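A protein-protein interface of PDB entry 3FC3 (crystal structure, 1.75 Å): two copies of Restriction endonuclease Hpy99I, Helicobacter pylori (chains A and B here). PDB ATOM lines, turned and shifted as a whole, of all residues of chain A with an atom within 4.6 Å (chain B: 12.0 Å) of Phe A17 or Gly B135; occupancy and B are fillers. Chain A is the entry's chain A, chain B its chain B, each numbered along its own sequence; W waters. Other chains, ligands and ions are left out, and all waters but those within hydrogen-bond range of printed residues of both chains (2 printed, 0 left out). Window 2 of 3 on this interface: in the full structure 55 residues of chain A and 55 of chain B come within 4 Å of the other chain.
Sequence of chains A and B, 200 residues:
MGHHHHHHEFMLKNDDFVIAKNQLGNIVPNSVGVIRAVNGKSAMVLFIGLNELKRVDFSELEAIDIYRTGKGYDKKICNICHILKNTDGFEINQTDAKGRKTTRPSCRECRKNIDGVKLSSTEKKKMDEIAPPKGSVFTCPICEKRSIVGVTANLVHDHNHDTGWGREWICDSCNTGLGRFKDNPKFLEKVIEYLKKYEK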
ATOM      1  N   ASP A  15       4.111  14.782 -24.601  1.00  0.00           N
ATOM      2  CA  ASP A  15       5.121  15.820 -24.793  1.00  0.00           C
ATOM      3  C   ASP A  15       4.585  17.227 -24.569  1.00  0.00           C
ATOM      4  O   ASP A  15       5.375  18.163 -24.496  1.00  0.00           O
ATOM      5  CB  ASP A  15       5.835  15.722 -26.137  1.00  0.00           C
ATOM      6  CG  ASP A  15       6.500  14.357 -26.371  1.00  0.00           C
ATOM      7  OD1 ASP A  15       7.079  13.757 -25.433  1.00  0.00           O
ATOM      8  OD2 ASP A  15       6.510  13.928 -27.531  1.00  0.00           O
ATOM      9  N   ASP A  16       3.266  17.375 -24.426  1.00  0.00           N
ATOM     10  CA  ASP A  16       2.664  18.671 -24.039  1.00  0.00           C
ATOM     11  C   ASP A  16       3.080  19.051 -22.609  1.00  0.00           C
ATOM     12  O   ASP A  16       3.314  18.190 -21.748  1.00  0.00           O
ATOM     13  CB  ASP A  16       1.140  18.611 -24.081  1.00  0.00           C
ATOM     14  CG  ASP A  16       0.555  18.619 -25.500  1.00  0.00           C
ATOM     15  OD1 ASP A  16       1.264  18.826 -26.520  1.00  0.00           O
ATOM     16  OD2 ASP A  16      -0.685  18.439 -25.561  1.00  0.00           O
ATOM     17  N   PHE A  17       3.119  20.355 -22.354  1.00  0.00           N
ATOM     18  CA  PHE A  17       3.379  20.882 -21.030  1.00  0.00           C
ATOM     19  C   PHE A  17       2.108  21.393 -20.359  1.00  0.00           C
ATOM     20  O   PHE A  17       1.242  21.996 -20.994  1.00  0.00           O
ATOM     21  CB  PHE A  17       4.414  22.001 -21.129  1.00  0.00           C
ATOM     22  CG  PHE A  17       5.780  21.488 -21.416  1.00  0.00           C
ATOM     23  CD1 PHE A  17       6.581  21.029 -20.375  1.00  0.00           C
ATOM     24  CD2 PHE A  17       6.241  21.408 -22.716  1.00  0.00           C
ATOM     25  CE1 PHE A  17       7.844  20.500 -20.632  1.00  0.00           C
ATOM     26  CE2 PHE A  17       7.504  20.910 -23.007  1.00  0.00           C
ATOM     27  CZ  PHE A  17       8.315  20.446 -21.936  1.00  0.00           C
ATOM     28  N   VAL A  18       2.030  21.112 -19.065  1.00  0.00           N
ATOM     29  CA  VAL A  18       0.897  21.482 -18.229  1.00  0.00           C
ATOM     30  C   VAL A  18       1.362  22.043 -16.915  1.00  0.00           C
ATOM     31  O   VAL A  18       2.506  21.838 -16.498  1.00  0.00           O
ATOM     32  CB  VAL A  18      -0.022  20.262 -17.950  1.00  0.00           C
ATOM     33  CG1 VAL A  18      -0.645  19.772 -19.249  1.00  0.00           C
ATOM     34  CG2 VAL A  18       0.746  19.165 -17.215  1.00  0.00           C
ATOM     35  N   VAL A  32       5.061  22.735 -13.104  1.00  0.00           N
ATOM     36  CA  VAL A  32       5.091  22.355 -14.517  1.00  0.00           C
ATOM     37  C   VAL A  32       5.424  20.878 -14.677  1.00  0.00           C
ATOM     38  O   VAL A  32       6.345  20.318 -14.031  1.00  0.00           O
ATOM     39  CB  VAL A  32       6.111  23.197 -15.291  1.00  0.00           C
ATOM     40  CG1 VAL A  32       6.188  22.756 -16.763  1.00  0.00           C
ATOM     41  CG2 VAL A  32       5.767  24.677 -15.177  1.00  0.00           C
ATOM     42  N   GLY A  33       4.636  20.239 -15.523  1.00  0.00           N
ATOM     43  CA  GLY A  33       4.854  18.866 -15.890  1.00  0.00           C
ATOM     44  C   GLY A  33       4.790  18.653 -17.377  1.00  0.00           C
ATOM     45  O   GLY A  33       4.274  19.491 -18.116  1.00  0.00           O
ATOM     46  N   VAL A  34       5.371  17.548 -17.811  1.00  0.00           N
ATOM     47  CA  VAL A  34       5.279  17.092 -19.189  1.00  0.00           C
ATOM     48  C   VAL A  34       4.456  15.802 -19.252  1.00  0.00           C
ATOM     49  O   VAL A  34       4.620  14.905 -18.402  1.00  0.00           O
ATOM     50  CB  VAL A  34       6.659  16.943 -19.836  1.00  0.00           C
ATOM     51  CG1 VAL A  34       7.497  15.934 -19.093  1.00  0.00           C
ATOM     52  CG2 VAL A  34       6.537  16.582 -21.308  1.00  0.00           C
ATOM     53  N   ILE A  48       8.477  18.086 -13.158  1.00  0.00           N
ATOM     54  CA  ILE A  48       9.913  18.155 -13.434  1.00  0.00           C
ATOM     55  C   ILE A  48      10.711  18.534 -12.178  1.00  0.00           C
ATOM     56  O   ILE A  48      11.773  17.964 -11.943  1.00  0.00           O
ATOM     57  CB  ILE A  48      10.188  19.153 -14.596  1.00  0.00           C
ATOM     58  CG1 ILE A  48       9.480  18.680 -15.885  1.00  0.00           C
ATOM     59  CG2 ILE A  48      11.677  19.342 -14.836  1.00  0.00           C
ATOM     60  CD1 ILE A  48       9.293  19.771 -16.928  1.00  0.00           C
ATOM     61  N   GLU A  62      -3.762  22.273 -16.550  1.00  0.00           N
ATOM     62  CA  GLU A  62      -3.957  23.358 -17.511  1.00  0.00           C
ATOM     63  C   GLU A  62      -2.771  23.374 -18.490  1.00  0.00           C
ATOM     64  O   GLU A  62      -1.622  23.465 -18.058  1.00  0.00           O
ATOM     65  CB  GLU A  62      -4.043  24.673 -16.751  1.00  0.00           C
ATOM     66  CG  GLU A  62      -4.209  25.877 -17.627  1.00  0.00           C
ATOM     67  CD  GLU A  62      -4.435  27.157 -16.832  1.00  0.00           C
ATOM     68  OE1 GLU A  62      -4.888  27.096 -15.655  1.00  0.00           O
ATOM     69  OE2 GLU A  62      -4.154  28.227 -17.400  1.00  0.00           O
ATOM     70  N   ALA A  63      -3.050  23.288 -19.791  1.00  0.00           N
ATOM     71  CA  ALA A  63      -1.984  23.396 -20.811  1.00  0.00           C
ATOM     72  C   ALA A  63      -1.330  24.771 -20.759  1.00  0.00           C
ATOM     73  O   ALA A  63      -2.003  25.804 -20.583  1.00  0.00           O
ATOM     74  CB  ALA A  63      -2.542  23.134 -22.232  1.00  0.00           C
ATOM     75  N   ILE A  64      -0.012  24.779 -20.930  1.00  0.00           N
ATOM     76  CA  ILE A  64       0.745  26.022 -21.041  1.00  0.00           C
ATOM     77  C   ILE A  64       1.628  25.980 -22.274  1.00  0.00           C
ATOM     78  O   ILE A  64       1.989  24.885 -22.768  1.00  0.00           O
ATOM     79  CB  ILE A  64       1.601  26.323 -19.780  1.00  0.00           C
ATOM     80  CG1 ILE A  64       2.667  25.253 -19.586  1.00  0.00           C
ATOM     81  CG2 ILE A  64       0.699  26.456 -18.551  1.00  0.00           C
ATOM     82  CD1 ILE A  64       3.844  25.711 -18.637  1.00  0.00           C
ATOM     83  N   ILE A  66       5.116  26.924 -23.296  1.00  0.00           N
ATOM     84  CA  ILE A  66       6.431  27.208 -22.708  1.00  0.00           C
ATOM     85  C   ILE A  66       7.170  28.360 -23.412  1.00  0.00           C
ATOM     86  O   ILE A  66       7.987  29.039 -22.795  1.00  0.00           O
ATOM     87  CB  ILE A  66       7.330  25.950 -22.653  1.00  0.00           C
ATOM     88  CG1 ILE A  66       7.574  25.368 -24.042  1.00  0.00           C
ATOM     89  CG2 ILE A  66       6.716  24.917 -21.714  1.00  0.00           C
ATOM     90  CD1 ILE A  66       8.563  24.162 -24.087  1.00  0.00           C
ATOM     91  N   TYR A  67       6.831  28.619 -24.675  1.00  0.00           N
ATOM     92  CA  TYR A  67       7.479  29.715 -25.403  1.00  0.00           C
ATOM     93  C   TYR A  67       6.850  31.090 -25.154  1.00  0.00           C
ATOM     94  O   TYR A  67       7.340  32.095 -25.662  1.00  0.00           O
ATOM     95  CB  TYR A  67       7.472  29.407 -26.868  1.00  0.00           C
ATOM     96  CG  TYR A  67       8.177  28.101 -27.140  1.00  0.00           C
ATOM     97  CD1 TYR A  67       9.505  27.911 -26.763  1.00  0.00           C
ATOM     98  CD2 TYR A  67       7.513  27.045 -27.735  1.00  0.00           C
ATOM     99  CE1 TYR A  67      10.142  26.700 -26.996  1.00  0.00           C
ATOM    100  CE2 TYR A  67       8.158  25.847 -27.980  1.00  0.00           C
ATOM    101  CZ  TYR A  67       9.458  25.681 -27.603  1.00  0.00           C
ATOM    102  OH  TYR A  67      10.091  24.472 -27.860  1.00  0.00           O
ATOM    103  N   ALA B 131      20.713  15.322 -31.123  1.00  0.00           N
ATOM    104  CA  ALA B 131      20.408  16.559 -30.398  1.00  0.00           C
ATOM    105  C   ALA B 131      19.084  16.424 -29.649  1.00  0.00           C
ATOM    106  O   ALA B 131      18.103  15.917 -30.217  1.00  0.00           O
ATOM    107  CB  ALA B 131      20.328  17.707 -31.337  1.00  0.00           C
ATOM    108  N   PRO B 132      19.055  16.842 -28.367  1.00  0.00           N
ATOM    109  CA  PRO B 132      17.774  16.915 -27.644  1.00  0.00           C
ATOM    110  C   PRO B 132      16.857  17.922 -28.356  1.00  0.00           C
ATOM    111  O   PRO B 132      17.290  19.038 -28.628  1.00  0.00           O
ATOM    112  CB  PRO B 132      18.186  17.434 -26.254  1.00  0.00           C
ATOM    113  CG  PRO B 132      19.630  17.157 -26.135  1.00  0.00           C
ATOM    114  CD  PRO B 132      20.196  17.225 -27.514  1.00  0.00           C
ATOM    115  N   PRO B 133      15.611  17.529 -28.676  1.00  0.00           N
ATOM    116  CA  PRO B 133      14.682  18.460 -29.308  1.00  0.00           C
ATOM    117  C   PRO B 133      14.443  19.686 -28.436  1.00  0.00           C
ATOM    118  O   PRO B 133      14.432  19.557 -27.219  1.00  0.00           O
ATOM    119  CB  PRO B 133      13.381  17.645 -29.433  1.00  0.00           C
ATOM    120  CG  PRO B 133      13.775  16.238 -29.309  1.00  0.00           C
ATOM    121  CD  PRO B 133      15.018  16.195 -28.478  1.00  0.00           C
ATOM    122  N   LYS B 134      14.282  20.851 -29.055  1.00  0.00           N
ATOM    123  CA  LYS B 134      13.845  22.053 -28.330  1.00  0.00           C
ATOM    124  C   LYS B 134      12.520  21.725 -27.634  1.00  0.00           C
ATOM    125  O   LYS B 134      11.663  21.071 -28.211  1.00  0.00           O
ATOM    126  CB  LYS B 134      13.625  23.228 -29.271  1.00  0.00           C
ATOM    127  CG  LYS B 134      13.757  24.583 -28.593  1.00  0.00           C
ATOM    128  CD  LYS B 134      13.161  25.723 -29.454  1.00  0.00           C
ATOM    129  CE  LYS B 134      13.837  27.068 -29.163  1.00  0.00           C
ATOM    130  NZ  LYS B 134      13.856  27.474 -27.711  1.00  0.00           N
ATOM    131  N   GLY B 135      12.383  22.141 -26.381  1.00  0.00           N
ATOM    132  CA  GLY B 135      11.177  21.869 -25.614  1.00  0.00           C
ATOM    133  C   GLY B 135      11.094  20.471 -25.032  1.00  0.00           C
ATOM    134  O   GLY B 135      10.063  20.092 -24.488  1.00  0.00           O
ATOM    135  N   SER B 136      12.142  19.662 -25.145  1.00  0.00           N
ATOM    136  CA  SER B 136      12.135  18.376 -24.459  1.00  0.00           C
ATOM    137  C   SER B 136      12.690  18.542 -23.027  1.00  0.00           C
ATOM    138  O   SER B 136      13.288  19.569 -22.715  1.00  0.00           O
ATOM    139  CB  SER B 136      12.948  17.366 -25.268  1.00  0.00           C
ATOM    140  OG  SER B 136      14.311  17.743 -25.312  1.00  0.00           O
ATOM    141  N   VAL B 137      12.439  17.570 -22.157  1.00  0.00           N
ATOM    142  CA  VAL B 137      12.975  17.564 -20.798  1.00  0.00           C
ATOM    143  C   VAL B 137      14.327  16.840 -20.809  1.00  0.00           C
ATOM    144  O   VAL B 137      14.429  15.680 -21.220  1.00  0.00           O
ATOM    145  CB  VAL B 137      11.996  16.911 -19.784  1.00  0.00           C
ATOM    146  CG1 VAL B 137      12.610  16.868 -18.410  1.00  0.00           C
ATOM    147  CG2 VAL B 137      10.651  17.689 -19.751  1.00  0.00           C
ATOM    148  N   PHE B 138      15.353  17.562 -20.370  1.00  0.00           N
ATOM    149  CA  PHE B 138      16.759  17.193 -20.521  1.00  0.00           C
ATOM    150  C   PHE B 138      17.366  17.171 -19.137  1.00  0.00           C
ATOM    151  O   PHE B 138      16.942  17.924 -18.251  1.00  0.00           O
ATOM    152  CB  PHE B 138      17.456  18.250 -21.383  1.00  0.00           C
ATOM    153  CG  PHE B 138      18.958  18.065 -21.523  1.00  0.00           C
ATOM    154  CD1 PHE B 138      19.474  17.153 -22.422  1.00  0.00           C
ATOM    155  CD2 PHE B 138      19.832  18.841 -20.778  1.00  0.00           C
ATOM    156  CE1 PHE B 138      20.854  17.010 -22.585  1.00  0.00           C
ATOM    157  CE2 PHE B 138      21.202  18.702 -20.919  1.00  0.00           C
ATOM    158  CZ  PHE B 138      21.716  17.780 -21.812  1.00  0.00           C
ATOM    159  N   THR B 139      18.333  16.287 -18.930  1.00  0.00           N
ATOM    160  CA  THR B 139      19.090  16.253 -17.689  1.00  0.00           C
ATOM    161  C   THR B 139      20.558  16.368 -18.109  1.00  0.00           C
ATOM    162  O   THR B 139      21.062  15.527 -18.856  1.00  0.00           O
ATOM    163  CB  THR B 139      18.886  14.959 -16.910  1.00  0.00           C
ATOM    164  OG1 THR B 139      17.480  14.726 -16.721  1.00  0.00           O
ATOM    165  CG2 THR B 139      19.560  15.037 -15.532  1.00  0.00           C
ATOM    166  N   ARG B 146      17.845  19.102 -14.262  1.00  0.00           N
ATOM    167  CA  ARG B 146      16.811  18.900 -15.256  1.00  0.00           C
ATOM    168  C   ARG B 146      16.413  20.263 -15.811  1.00  0.00           C
ATOM    169  O   ARG B 146      16.468  21.301 -15.106  1.00  0.00           O
ATOM    170  CB  ARG B 146      15.583  18.212 -14.643  1.00  0.00           C
ATOM    171  CG  ARG B 146      15.787  16.763 -14.259  1.00  0.00           C
ATOM    172  CD  ARG B 146      14.494  16.156 -13.703  1.00  0.00           C
ATOM    173  NE  ARG B 146      14.122  16.745 -12.420  1.00  0.00           N
ATOM    174  CZ  ARG B 146      14.713  16.476 -11.267  1.00  0.00           C
ATOM    175  NH1 ARG B 146      15.738  15.626 -11.197  1.00  0.00           N
ATOM    176  NH2 ARG B 146      14.295  17.081 -10.174  1.00  0.00           N
ATOM    177  N   SER B 147      16.050  20.275 -17.083  1.00  0.00           N
ATOM    178  CA  SER B 147      15.602  21.503 -17.710  1.00  0.00           C
ATOM    179  C   SER B 147      14.696  21.220 -18.893  1.00  0.00           C
ATOM    180  O   SER B 147      14.587  20.083 -19.339  1.00  0.00           O
ATOM    181  CB  SER B 147      16.798  22.319 -18.172  1.00  0.00           C
ATOM    182  OG  SER B 147      17.634  21.573 -19.063  1.00  0.00           O
ATOM    183  N   ILE B 148      14.056  22.272 -19.390  1.00  0.00           N
ATOM    184  CA  ILE B 148      13.269  22.200 -20.591  1.00  0.00           C
ATOM    185  C   ILE B 148      14.127  22.873 -21.651  1.00  0.00           C
ATOM    186  O   ILE B 148      14.463  24.054 -21.522  1.00  0.00           O
ATOM    187  CB  ILE B 148      11.943  22.940 -20.447  1.00  0.00           C
ATOM    188  CG1 ILE B 148      11.081  22.324 -19.337  1.00  0.00           C
ATOM    189  CG2 ILE B 148      11.173  23.000 -21.801  1.00  0.00           C
ATOM    190  CD1 ILE B 148       9.845  23.233 -18.937  1.00  0.00           C
ATOM    191  N   VAL B 149      14.498  22.125 -22.673  1.00  0.00           N
ATOM    192  CA  VAL B 149      15.510  22.594 -23.646  1.00  0.00           C
ATOM    193  C   VAL B 149      15.103  23.900 -24.333  1.00  0.00           C
ATOM    194  O   VAL B 149      14.043  23.974 -24.967  1.00  0.00           O
ATOM    195  CB  VAL B 149      15.820  21.528 -24.727  1.00  0.00           C
ATOM    196  CG1 VAL B 149      16.814  22.090 -25.711  1.00  0.00           C
ATOM    197  CG2 VAL B 149      16.416  20.270 -24.075  1.00  0.00           C
ATOM    198  N   GLY B 150      15.953  24.924 -24.182  1.00  0.00           N
ATOM    199  CA  GLY B 150      15.747  26.240 -24.764  1.00  0.00           C
ATOM    200  C   GLY B 150      14.768  27.131 -24.007  1.00  0.00           C
ATOM    201  O   GLY B 150      14.444  28.223 -24.461  1.00  0.00           O
ATOM    202  N   VAL B 151      14.260  26.659 -22.867  1.00  0.00           N
ATOM    203  CA  VAL B 151      13.292  27.415 -22.059  1.00  0.00           C
ATOM    204  C   VAL B 151      13.822  27.617 -20.645  1.00  0.00           C
ATOM    205  O   VAL B 151      13.921  28.749 -20.192  1.00  0.00           O
ATOM    206  CB  VAL B 151      11.904  26.724 -22.009  1.00  0.00           C
ATOM    207  CG1 VAL B 151      10.956  27.446 -21.024  1.00  0.00           C
ATOM    208  CG2 VAL B 151      11.309  26.645 -23.429  1.00  0.00           C
ATOM    209  N   THR B 152      14.199  26.544 -19.943  1.00  0.00           N
ATOM    210  CA  THR B 152      14.804  26.711 -18.612  1.00  0.00           C
ATOM    211  C   THR B 152      16.310  26.389 -18.569  1.00  0.00           C
ATOM    212  O   THR B 152      16.967  26.544 -17.537  1.00  0.00           O
ATOM    213  CB  THR B 152      14.036  25.913 -17.488  1.00  0.00           C
ATOM    214  OG1 THR B 152      14.114  24.497 -17.737  1.00  0.00           O
ATOM    215  CG2 THR B 152      12.596  26.349 -17.378  1.00  0.00           C
ATOM    216  N   ALA B 153      16.861  25.949 -19.687  1.00  0.00           N
ATOM    217  CA  ALA B 153      18.318  25.947 -19.876  1.00  0.00           C
ATOM    218  C   ALA B 153      18.604  25.857 -21.346  1.00  0.00           C
ATOM    219  O   ALA B 153      17.876  25.183 -22.089  1.00  0.00           O
ATOM    220  CB  ALA B 153      19.020  24.792 -19.117  1.00  0.00           C
ATOM    221  N   ASN B 154      19.656  26.554 -21.763  1.00  0.00           N
ATOM    222  CA  ASN B 154      20.135  26.500 -23.138  1.00  0.00           C
ATOM    223  C   ASN B 154      21.265  25.485 -23.227  1.00  0.00           C
ATOM    224  O   ASN B 154      22.164  25.451 -22.357  1.00  0.00           O
ATOM    225  CB  ASN B 154      20.641  27.853 -23.611  1.00  0.00           C
ATOM    226  CG  ASN B 154      19.512  28.866 -23.798  1.00  0.00           C
ATOM    227  OD1 ASN B 154      18.345  28.495 -23.989  1.00  0.00           O
ATOM    228  ND2 ASN B 154      19.862  30.132 -23.777  1.00  0.00           N
ATOM    229  N   LEU B 155      21.214  24.648 -24.253  1.00  0.00           N
ATOM    230  CA  LEU B 155      22.241  23.615 -24.463  1.00  0.00           C
ATOM    231  C   LEU B 155      23.213  23.923 -25.605  1.00  0.00           C
ATOM    232  O   LEU B 155      22.932  24.718 -26.519  1.00  0.00           O
ATOM    233  CB  LEU B 155      21.614  22.240 -24.733  1.00  0.00           C
ATOM    234  CG  LEU B 155      20.517  21.724 -23.822  1.00  0.00           C
ATOM    235  CD1 LEU B 155      20.129  20.336 -24.233  1.00  0.00           C
ATOM    236  CD2 LEU B 155      20.970  21.768 -22.380  1.00  0.00           C
ATOM    237  N   TRP B 169      26.212  16.805 -25.557  1.00  0.00           N
ATOM    238  CA  TRP B 169      25.290  17.911 -25.337  1.00  0.00           C
ATOM    239  C   TRP B 169      25.225  18.180 -23.848  1.00  0.00           C
ATOM    240  O   TRP B 169      24.917  17.276 -23.061  1.00  0.00           O
ATOM    241  CB  TRP B 169      23.909  17.563 -25.869  1.00  0.00           C
ATOM    242  CG  TRP B 169      23.821  17.639 -27.356  1.00  0.00           C
ATOM    243  CD1 TRP B 169      24.002  16.614 -28.262  1.00  0.00           C
ATOM    244  CD2 TRP B 169      23.512  18.796 -28.109  1.00  0.00           C
ATOM    245  NE1 TRP B 169      23.824  17.092 -29.544  1.00  0.00           N
ATOM    246  CE2 TRP B 169      23.519  18.428 -29.472  1.00  0.00           C
ATOM    247  CE3 TRP B 169      23.239  20.127 -27.765  1.00  0.00           C
ATOM    248  CZ2 TRP B 169      23.270  19.348 -30.489  1.00  0.00           C
ATOM    249  CZ3 TRP B 169      22.989  21.042 -28.779  1.00  0.00           C
ATOM    250  CH2 TRP B 169      22.988  20.647 -30.123  1.00  0.00           C
HETATM  251  O   HOH W   1       8.720  22.747 -28.949  1.00  0.00           O
HETATM  252  O   HOH W   2       8.244  17.983 -24.591  1.00  0.00           O
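The backbone carbonyl oxygen of Ile A48 lies within hydrogen-bond range of the guanidinium group of Arg B146.
Among the printed residues, merely in contact across the chains: Phe A17 with Gly B135 (3.1 Å), Phe A17 with Ile B148 (3.8 Å), Val A34 with Val B137 (3.7 Å), Ile A48 with Val B137 (3.8 Å), Ile A48 with Ile B148 (3.9 Å), Ile A66 with Gly B135 (3.8 Å), Ile A66 with Ile B148 (3.7 Å), Ile A66 with Val B151 (3.8 Å), Tyr A67 with Lys B134 (3.7 Å), Tyr A67 with Gly B135 (3.6 Å) and Tyr A67 with Val B151 (3.8 Å).
Water W1 bridges the side-chain hydroxyl (OH) of Tyr A67 and the backbone carbonyl oxygen (O) of Lys B134.
Water W2 bridges the backbone carbonyl oxygen (O) of Gly B135 (2.8 Å) and the backbone carbonyl oxygen (O) of Asp A15 (2.9 Å).
Of the 13 printed residues of chain A, 5 touch a printed residue of chain B.
Hydrophobic or aromatic side chains of chain B within 4 Å of the printed part of chain A: Val B137, Ile B148 and Val B151.
Among the printed residues, no Asp or Glu carboxylate lies within 4 Å of a Lys or Arg side-chain nitrogen of the other chain.
The side-chain amino group (NZ) of Lys B134 is in hydrogen-bond range of the backbone carbonyl oxygen (O) of Gly B150.
The backbone carbonyl oxygen of Phe A17 lies within hydrogen-bond range of the backbone NH of Ile A64, 3.1 Å away.
O of Val A32 sits at hydrogen-bond distance from N of Ile A48 (3.2 Å).
The backbone NH (N) of Gly B135 sits at hydrogen-bond distance from the backbone carbonyl oxygen (O) of Val B149 (2.8 Å).
The backbone NH (N) of Ile B148 sits at hydrogen-bond distance from the side-chain hydroxyl (OG1) of Thr B152, at 2.8 Å.
No position is printed for both chains.
Gly B135 touches three residues of chain A.
No residue of chain B comes within 4 Å of Asp A15.
No residue of chain B comes within 4 Å of Asp A16.
No residue of chain B comes within 4 Å of Val A18.
No residue of chain B comes within 4 Å of Val A32.
No residue of chain B comes within 4 Å of Gly A33.
Of chain B, only Val B137 comes within 4 Å of Val A34.
Ala A63 touches none of the printed residues of chain B.
Of chain B, only Gly B135 (3.8 Å), Ile B148 (3.7 Å) and Val B151 (3.8 Å) come within 4 Å of Ile A66.
Printed residues of chain B within 4 Å of Tyr A67: Lys B134 (3.7 Å), Gly B135 (3.6 Å) and Val B151 (3.8 Å).
Of the printed residues of chain A, Lys B134 touches Tyr A67.
The nearest printed residue of chain A that does not touch Gly B135 is Asp A15 (5.1 Å).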
